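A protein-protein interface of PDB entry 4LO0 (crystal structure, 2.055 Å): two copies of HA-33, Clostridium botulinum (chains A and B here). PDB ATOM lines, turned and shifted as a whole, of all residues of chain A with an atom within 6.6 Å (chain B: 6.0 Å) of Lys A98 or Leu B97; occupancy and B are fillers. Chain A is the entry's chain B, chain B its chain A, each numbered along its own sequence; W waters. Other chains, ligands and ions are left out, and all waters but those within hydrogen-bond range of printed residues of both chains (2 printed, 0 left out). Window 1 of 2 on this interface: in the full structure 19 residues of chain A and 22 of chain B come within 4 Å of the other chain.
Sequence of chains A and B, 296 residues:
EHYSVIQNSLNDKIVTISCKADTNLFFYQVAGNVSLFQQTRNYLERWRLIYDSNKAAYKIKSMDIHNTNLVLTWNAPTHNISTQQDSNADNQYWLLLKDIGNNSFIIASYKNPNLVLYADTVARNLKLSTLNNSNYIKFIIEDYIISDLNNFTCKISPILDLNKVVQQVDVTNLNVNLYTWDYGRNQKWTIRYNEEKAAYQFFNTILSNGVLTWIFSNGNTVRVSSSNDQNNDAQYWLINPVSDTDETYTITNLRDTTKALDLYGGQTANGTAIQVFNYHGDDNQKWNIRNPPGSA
Of the printed residues of chain B, Lys A98 touches Leu B96 (3.6 Å), Leu B97 (3.4 Å), Lys B98 (2.6 Å) and Ile B100 (3.9 Å). Of chain A, only Lys A98 (3.4 Å) and Asp A99 (3.9 Å) come within 4 Å of Leu B97. Of the printed residues of chain B, Ile A100 touches Leu B96 (3.2 Å), Lys B98 (3.97 Å) and Phe B105 (3.8 Å). Of the printed residues of chain B, Phe A105 touches Ile B100. Of the printed residues of chain B, Asp A99 touches Leu B96 and Leu B97. Printed residues of chain B within 4 Å of Leu A96: Lys B98, Asp B99 and Ile B100. The nearest printed residue of chain A that does not touch Leu B97 is Ile A106 (4.1 Å). The nearest printed residue of chain B that does not touch Leu A97 is Leu B97 (4.1 Å).
Water W2 bridges OD1 of Asp A99 (2.7 Å) and N of Leu B96 (3.2 Å). Water W1 bridges OD1 of Asp B99 (2.8 Å) and N of Leu A96 (3.0 Å).
Of the 11 printed residues of chain A, 6 touch a printed residue of chain B. Among the printed residues, no Asp or Glu carboxylate lies within 4 Å of a Lys or Arg side-chain nitrogen of the other chain.
CA of Asp B99 touches O of Leu A96, 3.8 Å away. Lys B98 touches Leu A97 (O to CA, 3.3 Å). Leu A97 touches Asp B99 (CD2 to CA, 3.8 Å). O of Lys A98 touches O of Leu B96 (3.6 Å). Lys A98 touches Leu B97 (O to CA, 3.4 Å). Asp A99 touches Leu B96. CA of Asp A99 touches CD2 of Leu B97 (3.9 Å). Ile A100 touches Lys B98. Phe B105 touches Ile A100. Ile B100 touches Phe A105 (CG1 to CE1, 3.8 Å).
The backbone NH of Ile A106 is in hydrogen-bond range of the backbone carbonyl oxygen of Leu A97 (2.8 Å). The side-chain amino group (NZ) of Lys A98 is in hydrogen-bond range of the side-chain amide oxygen (OD1) of Asn A103 (3.1 Å). N of Asp B99 is in hydrogen-bond range of O of Ser B104, at 2.9 Å. O of Ser A104 sits at hydrogen-bond distance from N of Asp A99 (2.8 Å). The backbone carbonyl oxygen (O) of Leu B97 lies within hydrogen-bond range of the backbone NH (N) of Ile B106, 2.8 Å away.
The backbone NH (N) of Lys B98 is in hydrogen-bond range of the backbone carbonyl oxygen (O) of Lys A98. O of Leu B96 is in hydrogen-bond range of N of Ile A100 (3.2 Å). The backbone NH of Ile B100 lies within hydrogen-bond range of the backbone carbonyl oxygen of Leu A96, 3.2 Å away. The backbone carbonyl oxygen (O) of Leu A96 lies close to the backbone carbonyl oxygen (O) of Lys B98, 3.4 Å away.
Leu A97 touches Asp B99, and with the chains exchanged Asp A99 touches Leu B97. Lys B98 touches its own counterpart, Lys A98. Lys A98 touches Ile B100, and with the chains exchanged Ile A100 touches Lys B98. Ile A100 touches Phe B105, and with the chains exchanged Phe A105 touches Ile B100. 8 positions are printed for both chains. Of the 15 pairs that touch across the chains among the printed residues, 15 have their exchanged pair printed and touching as well.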
ATOM      1  N   LEU A  96     -15.309   3.525   0.418  1.00  0.00           N
ATOM      2  CA  LEU A  96     -15.515   4.576   1.403  1.00  0.00           C
ATOM      3  C   LEU A  96     -16.424   3.984   2.480  1.00  0.00           C
ATOM      4  O   LEU A  96     -17.650   3.822   2.293  1.00  0.00           O
ATOM      5  CB  LEU A  96     -16.148   5.808   0.768  1.00  0.00           C
ATOM      6  CG  LEU A  96     -15.260   6.457  -0.319  1.00  0.00           C
ATOM      7  CD1 LEU A  96     -15.925   7.709  -0.843  1.00  0.00           C
ATOM      8  CD2 LEU A  96     -13.854   6.791   0.185  1.00  0.00           C
ATOM      9  N   LEU A  97     -15.811   3.647   3.601  1.00  0.00           N
ATOM     10  CA  LEU A  97     -16.525   3.007   4.693  1.00  0.00           C
ATOM     11  C   LEU A  97     -16.750   4.016   5.793  1.00  0.00           C
ATOM     12  O   LEU A  97     -15.798   4.450   6.455  1.00  0.00           O
ATOM     13  CB  LEU A  97     -15.704   1.847   5.212  1.00  0.00           C
ATOM     14  CG  LEU A  97     -15.280   0.864   4.130  1.00  0.00           C
ATOM     15  CD1 LEU A  97     -14.352  -0.209   4.785  1.00  0.00           C
ATOM     16  CD2 LEU A  97     -16.484   0.224   3.447  1.00  0.00           C
ATOM     17  N   LYS A  98     -18.009   4.385   6.012  1.00  0.00           N
ATOM     18  CA  LYS A  98     -18.299   5.353   7.043  1.00  0.00           C
ATOM     19  C   LYS A  98     -18.475   4.656   8.383  1.00  0.00           C
ATOM     20  O   LYS A  98     -19.373   3.801   8.545  1.00  0.00           O
ATOM     21  CB  LYS A  98     -19.566   6.147   6.722  1.00  0.00           C
ATOM     22  CG  LYS A  98     -19.742   7.351   7.626  1.00  0.00           C
ATOM     23  CD  LYS A  98     -20.919   8.219   7.218  1.00  0.00           C
ATOM     24  CE  LYS A  98     -20.724   9.630   7.755  1.00  0.00           C
ATOM     25  NZ  LYS A  98     -22.036  10.278   8.088  1.00  0.00           N
ATOM     26  N   ASP A  99     -17.610   5.032   9.327  1.00  0.00           N
ATOM     27  CA  ASP A  99     -17.643   4.543  10.708  1.00  0.00           C
ATOM     28  C   ASP A  99     -18.753   5.256  11.468  1.00  0.00           C
ATOM     29  O   ASP A  99     -18.556   6.364  11.982  1.00  0.00           O
ATOM     30  CB  ASP A  99     -16.293   4.809  11.394  1.00  0.00           C
ATOM     31  CG  ASP A  99     -16.167   4.116  12.745  1.00  0.00           C
ATOM     32  OD1 ASP A  99     -17.185   3.680  13.339  1.00  0.00           O
ATOM     33  OD2 ASP A  99     -15.029   4.007  13.235  1.00  0.00           O
ATOM     34  N   ILE A 100     -19.908   4.602  11.565  1.00  0.00           N
ATOM     35  CA  ILE A 100     -21.091   5.229  12.170  1.00  0.00           C
ATOM     36  C   ILE A 100     -20.889   5.500  13.662  1.00  0.00           C
ATOM     37  O   ILE A 100     -20.251   4.720  14.382  1.00  0.00           O
ATOM     38  CB  ILE A 100     -22.378   4.395  11.928  1.00  0.00           C
ATOM     39  CG1 ILE A 100     -22.488   4.080  10.447  1.00  0.00           C
ATOM     40  CG2 ILE A 100     -23.619   5.189  12.328  1.00  0.00           C
ATOM     41  CD1 ILE A 100     -22.592   5.328   9.591  1.00  0.00           C
ATOM     42  N   GLY A 101     -21.400   6.631  14.114  1.00  0.00           N
ATOM     43  CA  GLY A 101     -21.185   7.061  15.478  1.00  0.00           C
ATOM     44  C   GLY A 101     -19.924   7.896  15.618  1.00  0.00           C
ATOM     45  O   GLY A 101     -19.820   8.720  16.530  1.00  0.00           O
ATOM     46  N   ASN A 103     -18.566   9.423  12.761  1.00  0.00           N
ATOM     47  CA  ASN A 103     -18.637  10.399  11.679  1.00  0.00           C
ATOM     48  C   ASN A 103     -17.288  10.582  10.978  1.00  0.00           C
ATOM     49  O   ASN A 103     -16.860  11.697  10.701  1.00  0.00           O
ATOM     50  CB  ASN A 103     -19.151  11.747  12.184  1.00  0.00           C
ATOM     51  CG  ASN A 103     -19.853  12.536  11.103  1.00  0.00           C
ATOM     52  OD1 ASN A 103     -20.609  11.968  10.308  1.00  0.00           O
ATOM     53  ND2 ASN A 103     -19.594  13.850  11.047  1.00  0.00           N
ATOM     54  N   SER A 104     -16.614   9.473  10.710  1.00  0.00           N
ATOM     55  CA  SER A 104     -15.356   9.507  10.007  1.00  0.00           C
ATOM     56  C   SER A 104     -15.356   8.326   9.067  1.00  0.00           C
ATOM     57  O   SER A 104     -16.208   7.415   9.179  1.00  0.00           O
ATOM     58  CB  SER A 104     -14.187   9.425  10.987  1.00  0.00           C
ATOM     59  OG  SER A 104     -14.182   8.159  11.631  1.00  0.00           O
ATOM     60  N   PHE A 105     -14.410   8.341   8.138  1.00  0.00           N
ATOM     61  CA  PHE A 105     -14.358   7.346   7.098  1.00  0.00           C
ATOM     62  C   PHE A 105     -13.072   6.562   7.159  1.00  0.00           C
ATOM     63  O   PHE A 105     -11.987   7.097   7.436  1.00  0.00           O
ATOM     64  CB  PHE A 105     -14.415   8.004   5.718  1.00  0.00           C
ATOM     65  CG  PHE A 105     -15.803   8.363   5.255  1.00  0.00           C
ATOM     66  CD1 PHE A 105     -16.512   7.489   4.446  1.00  0.00           C
ATOM     67  CD2 PHE A 105     -16.382   9.596   5.598  1.00  0.00           C
ATOM     68  CE1 PHE A 105     -17.781   7.814   3.984  1.00  0.00           C
ATOM     69  CE2 PHE A 105     -17.670   9.931   5.159  1.00  0.00           C
ATOM     70  CZ  PHE A 105     -18.371   9.043   4.340  1.00  0.00           C
ATOM     71  N   ILE A 106     -13.191   5.289   6.835  1.00  0.00           N
ATOM     72  CA  ILE A 106     -12.019   4.510   6.498  1.00  0.00           C
ATOM     73  C   ILE A 106     -12.028   4.368   4.985  1.00  0.00           C
ATOM     74  O   ILE A 106     -13.099   4.229   4.358  1.00  0.00           O
ATOM     75  CB  ILE A 106     -12.044   3.140   7.217  1.00  0.00           C
ATOM     76  CG1 ILE A 106     -11.782   3.384   8.707  1.00  0.00           C
ATOM     77  CG2 ILE A 106     -10.988   2.207   6.644  1.00  0.00           C
ATOM     78  CD1 ILE A 106     -12.134   2.213   9.595  1.00  0.00           C
ATOM     79  N   LEU A 131      -6.317  -2.774   8.966  1.00  0.00           N
ATOM     80  CA  LEU A 131      -7.306  -2.098   9.811  1.00  0.00           C
ATOM     81  C   LEU A 131      -6.943  -2.195  11.276  1.00  0.00           C
ATOM     82  O   LEU A 131      -6.531  -3.243  11.754  1.00  0.00           O
ATOM     83  CB  LEU A 131      -8.661  -2.779   9.688  1.00  0.00           C
ATOM     84  CG  LEU A 131      -9.742  -2.291   8.756  1.00  0.00           C
ATOM     85  CD1 LEU A 131     -10.000  -0.806   9.000  1.00  0.00           C
ATOM     86  CD2 LEU A 131      -9.292  -2.572   7.353  1.00  0.00           C
ATOM     87  N   LEU B  95     -17.129  -2.669  15.104  1.00  0.00           N
ATOM     88  CA  LEU B  95     -17.160  -1.413  14.359  1.00  0.00           C
ATOM     89  C   LEU B  95     -18.183  -1.603  13.266  1.00  0.00           C
ATOM     90  O   LEU B  95     -18.125  -2.585  12.542  1.00  0.00           O
ATOM     91  CB  LEU B  95     -15.796  -1.122  13.706  1.00  0.00           C
ATOM     92  CG  LEU B  95     -14.546  -1.237  14.564  1.00  0.00           C
ATOM     93  CD1 LEU B  95     -13.288  -0.773  13.714  1.00  0.00           C
ATOM     94  CD2 LEU B  95     -14.676  -0.447  15.860  1.00  0.00           C
ATOM     95  N   LEU B  96     -19.139  -0.691  13.155  1.00  0.00           N
ATOM     96  CA  LEU B  96     -20.126  -0.779  12.090  1.00  0.00           C
ATOM     97  C   LEU B  96     -19.687   0.211  11.015  1.00  0.00           C
ATOM     98  O   LEU B  96     -19.766   1.434  11.192  1.00  0.00           O
ATOM     99  CB  LEU B  96     -21.512  -0.419  12.599  1.00  0.00           C
ATOM    100  CG  LEU B  96     -21.952  -1.308  13.766  1.00  0.00           C
ATOM    101  CD1 LEU B  96     -23.375  -0.885  14.211  1.00  0.00           C
ATOM    102  CD2 LEU B  96     -21.917  -2.747  13.367  1.00  0.00           C
ATOM    103  N   LEU B  97     -19.207  -0.340   9.912  1.00  0.00           N
ATOM    104  CA  LEU B  97     -18.594   0.477   8.868  1.00  0.00           C
ATOM    105  C   LEU B  97     -19.532   0.463   7.689  1.00  0.00           C
ATOM    106  O   LEU B  97     -19.702  -0.562   7.020  1.00  0.00           O
ATOM    107  CB  LEU B  97     -17.243  -0.113   8.469  1.00  0.00           C
ATOM    108  CG  LEU B  97     -16.278  -0.294   9.647  1.00  0.00           C
ATOM    109  CD1 LEU B  97     -14.982  -1.014   9.209  1.00  0.00           C
ATOM    110  CD2 LEU B  97     -15.971   1.043  10.293  1.00  0.00           C
ATOM    111  N   LYS B  98     -20.168   1.591   7.440  1.00  0.00           N
ATOM    112  CA  LYS B  98     -21.166   1.646   6.361  1.00  0.00           C
ATOM    113  C   LYS B  98     -20.508   1.931   5.011  1.00  0.00           C
ATOM    114  O   LYS B  98     -19.859   2.974   4.781  1.00  0.00           O
ATOM    115  CB  LYS B  98     -22.270   2.673   6.653  1.00  0.00           C
ATOM    116  CG  LYS B  98     -23.535   2.555   5.758  1.00  0.00           C
ATOM    117  CD  LYS B  98     -24.511   3.715   6.051  1.00  0.00           C
ATOM    118  CE  LYS B  98     -25.918   3.447   5.509  1.00  0.00           C
ATOM    119  NZ  LYS B  98     -26.887   4.529   5.901  1.00  0.00           N
ATOM    120  N   ASP B  99     -20.675   0.971   4.124  1.00  0.00           N
ATOM    121  CA  ASP B  99     -20.164   1.040   2.775  1.00  0.00           C
ATOM    122  C   ASP B  99     -21.096   1.942   1.982  1.00  0.00           C
ATOM    123  O   ASP B  99     -22.186   1.519   1.561  1.00  0.00           O
ATOM    124  CB  ASP B  99     -20.131  -0.392   2.230  1.00  0.00           C
ATOM    125  CG  ASP B  99     -19.398  -0.513   0.910  1.00  0.00           C
ATOM    126  OD1 ASP B  99     -19.243   0.503   0.196  1.00  0.00           O
ATOM    127  OD2 ASP B  99     -18.984  -1.642   0.584  1.00  0.00           O
ATOM    128  N   ILE B 100     -20.716   3.210   1.836  1.00  0.00           N
ATOM    129  CA  ILE B 100     -21.644   4.189   1.260  1.00  0.00           C
ATOM    130  C   ILE B 100     -21.897   3.903  -0.230  1.00  0.00           C
ATOM    131  O   ILE B 100     -20.981   3.522  -0.984  1.00  0.00           O
ATOM    132  CB  ILE B 100     -21.142   5.649   1.468  1.00  0.00           C
ATOM    133  CG1 ILE B 100     -20.951   5.931   2.960  1.00  0.00           C
ATOM    134  CG2 ILE B 100     -22.104   6.668   0.862  1.00  0.00           C
ATOM    135  CD1 ILE B 100     -22.174   5.652   3.826  1.00  0.00           C
ATOM    136  N   SER B 104     -24.805  -1.133   2.686  1.00  0.00           N
ATOM    137  CA  SER B 104     -24.511  -2.337   3.458  1.00  0.00           C
ATOM    138  C   SER B 104     -23.409  -2.014   4.431  1.00  0.00           C
ATOM    139  O   SER B 104     -22.803  -0.926   4.341  1.00  0.00           O
ATOM    140  CB  SER B 104     -24.133  -3.488   2.535  1.00  0.00           C
ATOM    141  OG  SER B 104     -22.923  -3.237   1.847  1.00  0.00           O
ATOM    142  N   PHE B 105     -23.157  -2.928   5.362  1.00  0.00           N
ATOM    143  CA  PHE B 105     -22.188  -2.689   6.423  1.00  0.00           C
ATOM    144  C   PHE B 105     -21.138  -3.778   6.417  1.00  0.00           C
ATOM    145  O   PHE B 105     -21.433  -4.961   6.208  1.00  0.00           O
ATOM    146  CB  PHE B 105     -22.831  -2.734   7.819  1.00  0.00           C
ATOM    147  CG  PHE B 105     -23.591  -1.485   8.194  1.00  0.00           C
ATOM    148  CD1 PHE B 105     -23.015  -0.525   9.016  1.00  0.00           C
ATOM    149  CD2 PHE B 105     -24.886  -1.280   7.733  1.00  0.00           C
ATOM    150  CE1 PHE B 105     -23.731   0.624   9.368  1.00  0.00           C
ATOM    151  CE2 PHE B 105     -25.607  -0.126   8.072  1.00  0.00           C
ATOM    152  CZ  PHE B 105     -25.035   0.823   8.882  1.00  0.00           C
ATOM    153  N   ILE B 106     -19.913  -3.371   6.700  1.00  0.00           N
ATOM    154  CA  ILE B 106     -18.893  -4.320   7.073  1.00  0.00           C
ATOM    155  C   ILE B 106     -18.816  -4.249   8.584  1.00  0.00           C
ATOM    156  O   ILE B 106     -18.836  -3.166   9.173  1.00  0.00           O
ATOM    157  CB  ILE B 106     -17.528  -3.979   6.410  1.00  0.00           C
ATOM    158  CG1 ILE B 106     -17.594  -4.323   4.921  1.00  0.00           C
ATOM    159  CG2 ILE B 106     -16.381  -4.762   7.093  1.00  0.00           C
ATOM    160  CD1 ILE B 106     -16.304  -3.853   4.093  1.00  0.00           C
ATOM    161  N   ILE B 107     -18.762  -5.403   9.228  1.00  0.00           N
ATOM    162  CA  ILE B 107     -18.836  -5.409  10.686  1.00  0.00           C
ATOM    163  C   ILE B 107     -17.531  -5.983  11.203  1.00  0.00           C
ATOM    164  O   ILE B 107     -17.275  -7.201  11.107  1.00  0.00           O
ATOM    165  CB  ILE B 107     -20.043  -6.243  11.169  1.00  0.00           C
ATOM    166  CG1 ILE B 107     -21.334  -5.653  10.589  1.00  0.00           C
ATOM    167  CG2 ILE B 107     -20.108  -6.325  12.719  1.00  0.00           C
ATOM    168  CD1 ILE B 107     -22.611  -6.410  10.986  1.00  0.00           C
ATOM    169  N   ALA B 108     -16.695  -5.101  11.735  1.00  0.00           N
ATOM    170  CA  ALA B 108     -15.328  -5.478  12.092  1.00  0.00           C
ATOM    171  C   ALA B 108     -15.179  -5.672  13.586  1.00  0.00           C
ATOM    172  O   ALA B 108     -15.750  -4.925  14.374  1.00  0.00           O
ATOM    173  CB  ALA B 108     -14.365  -4.413  11.637  1.00  0.00           C
HETATM  174  O   HOH W   1     -17.512   2.252  -1.205  1.00  0.00           O
HETATM  175  O   HOH W   2     -18.263   1.805  14.962  1.00  0.00           O
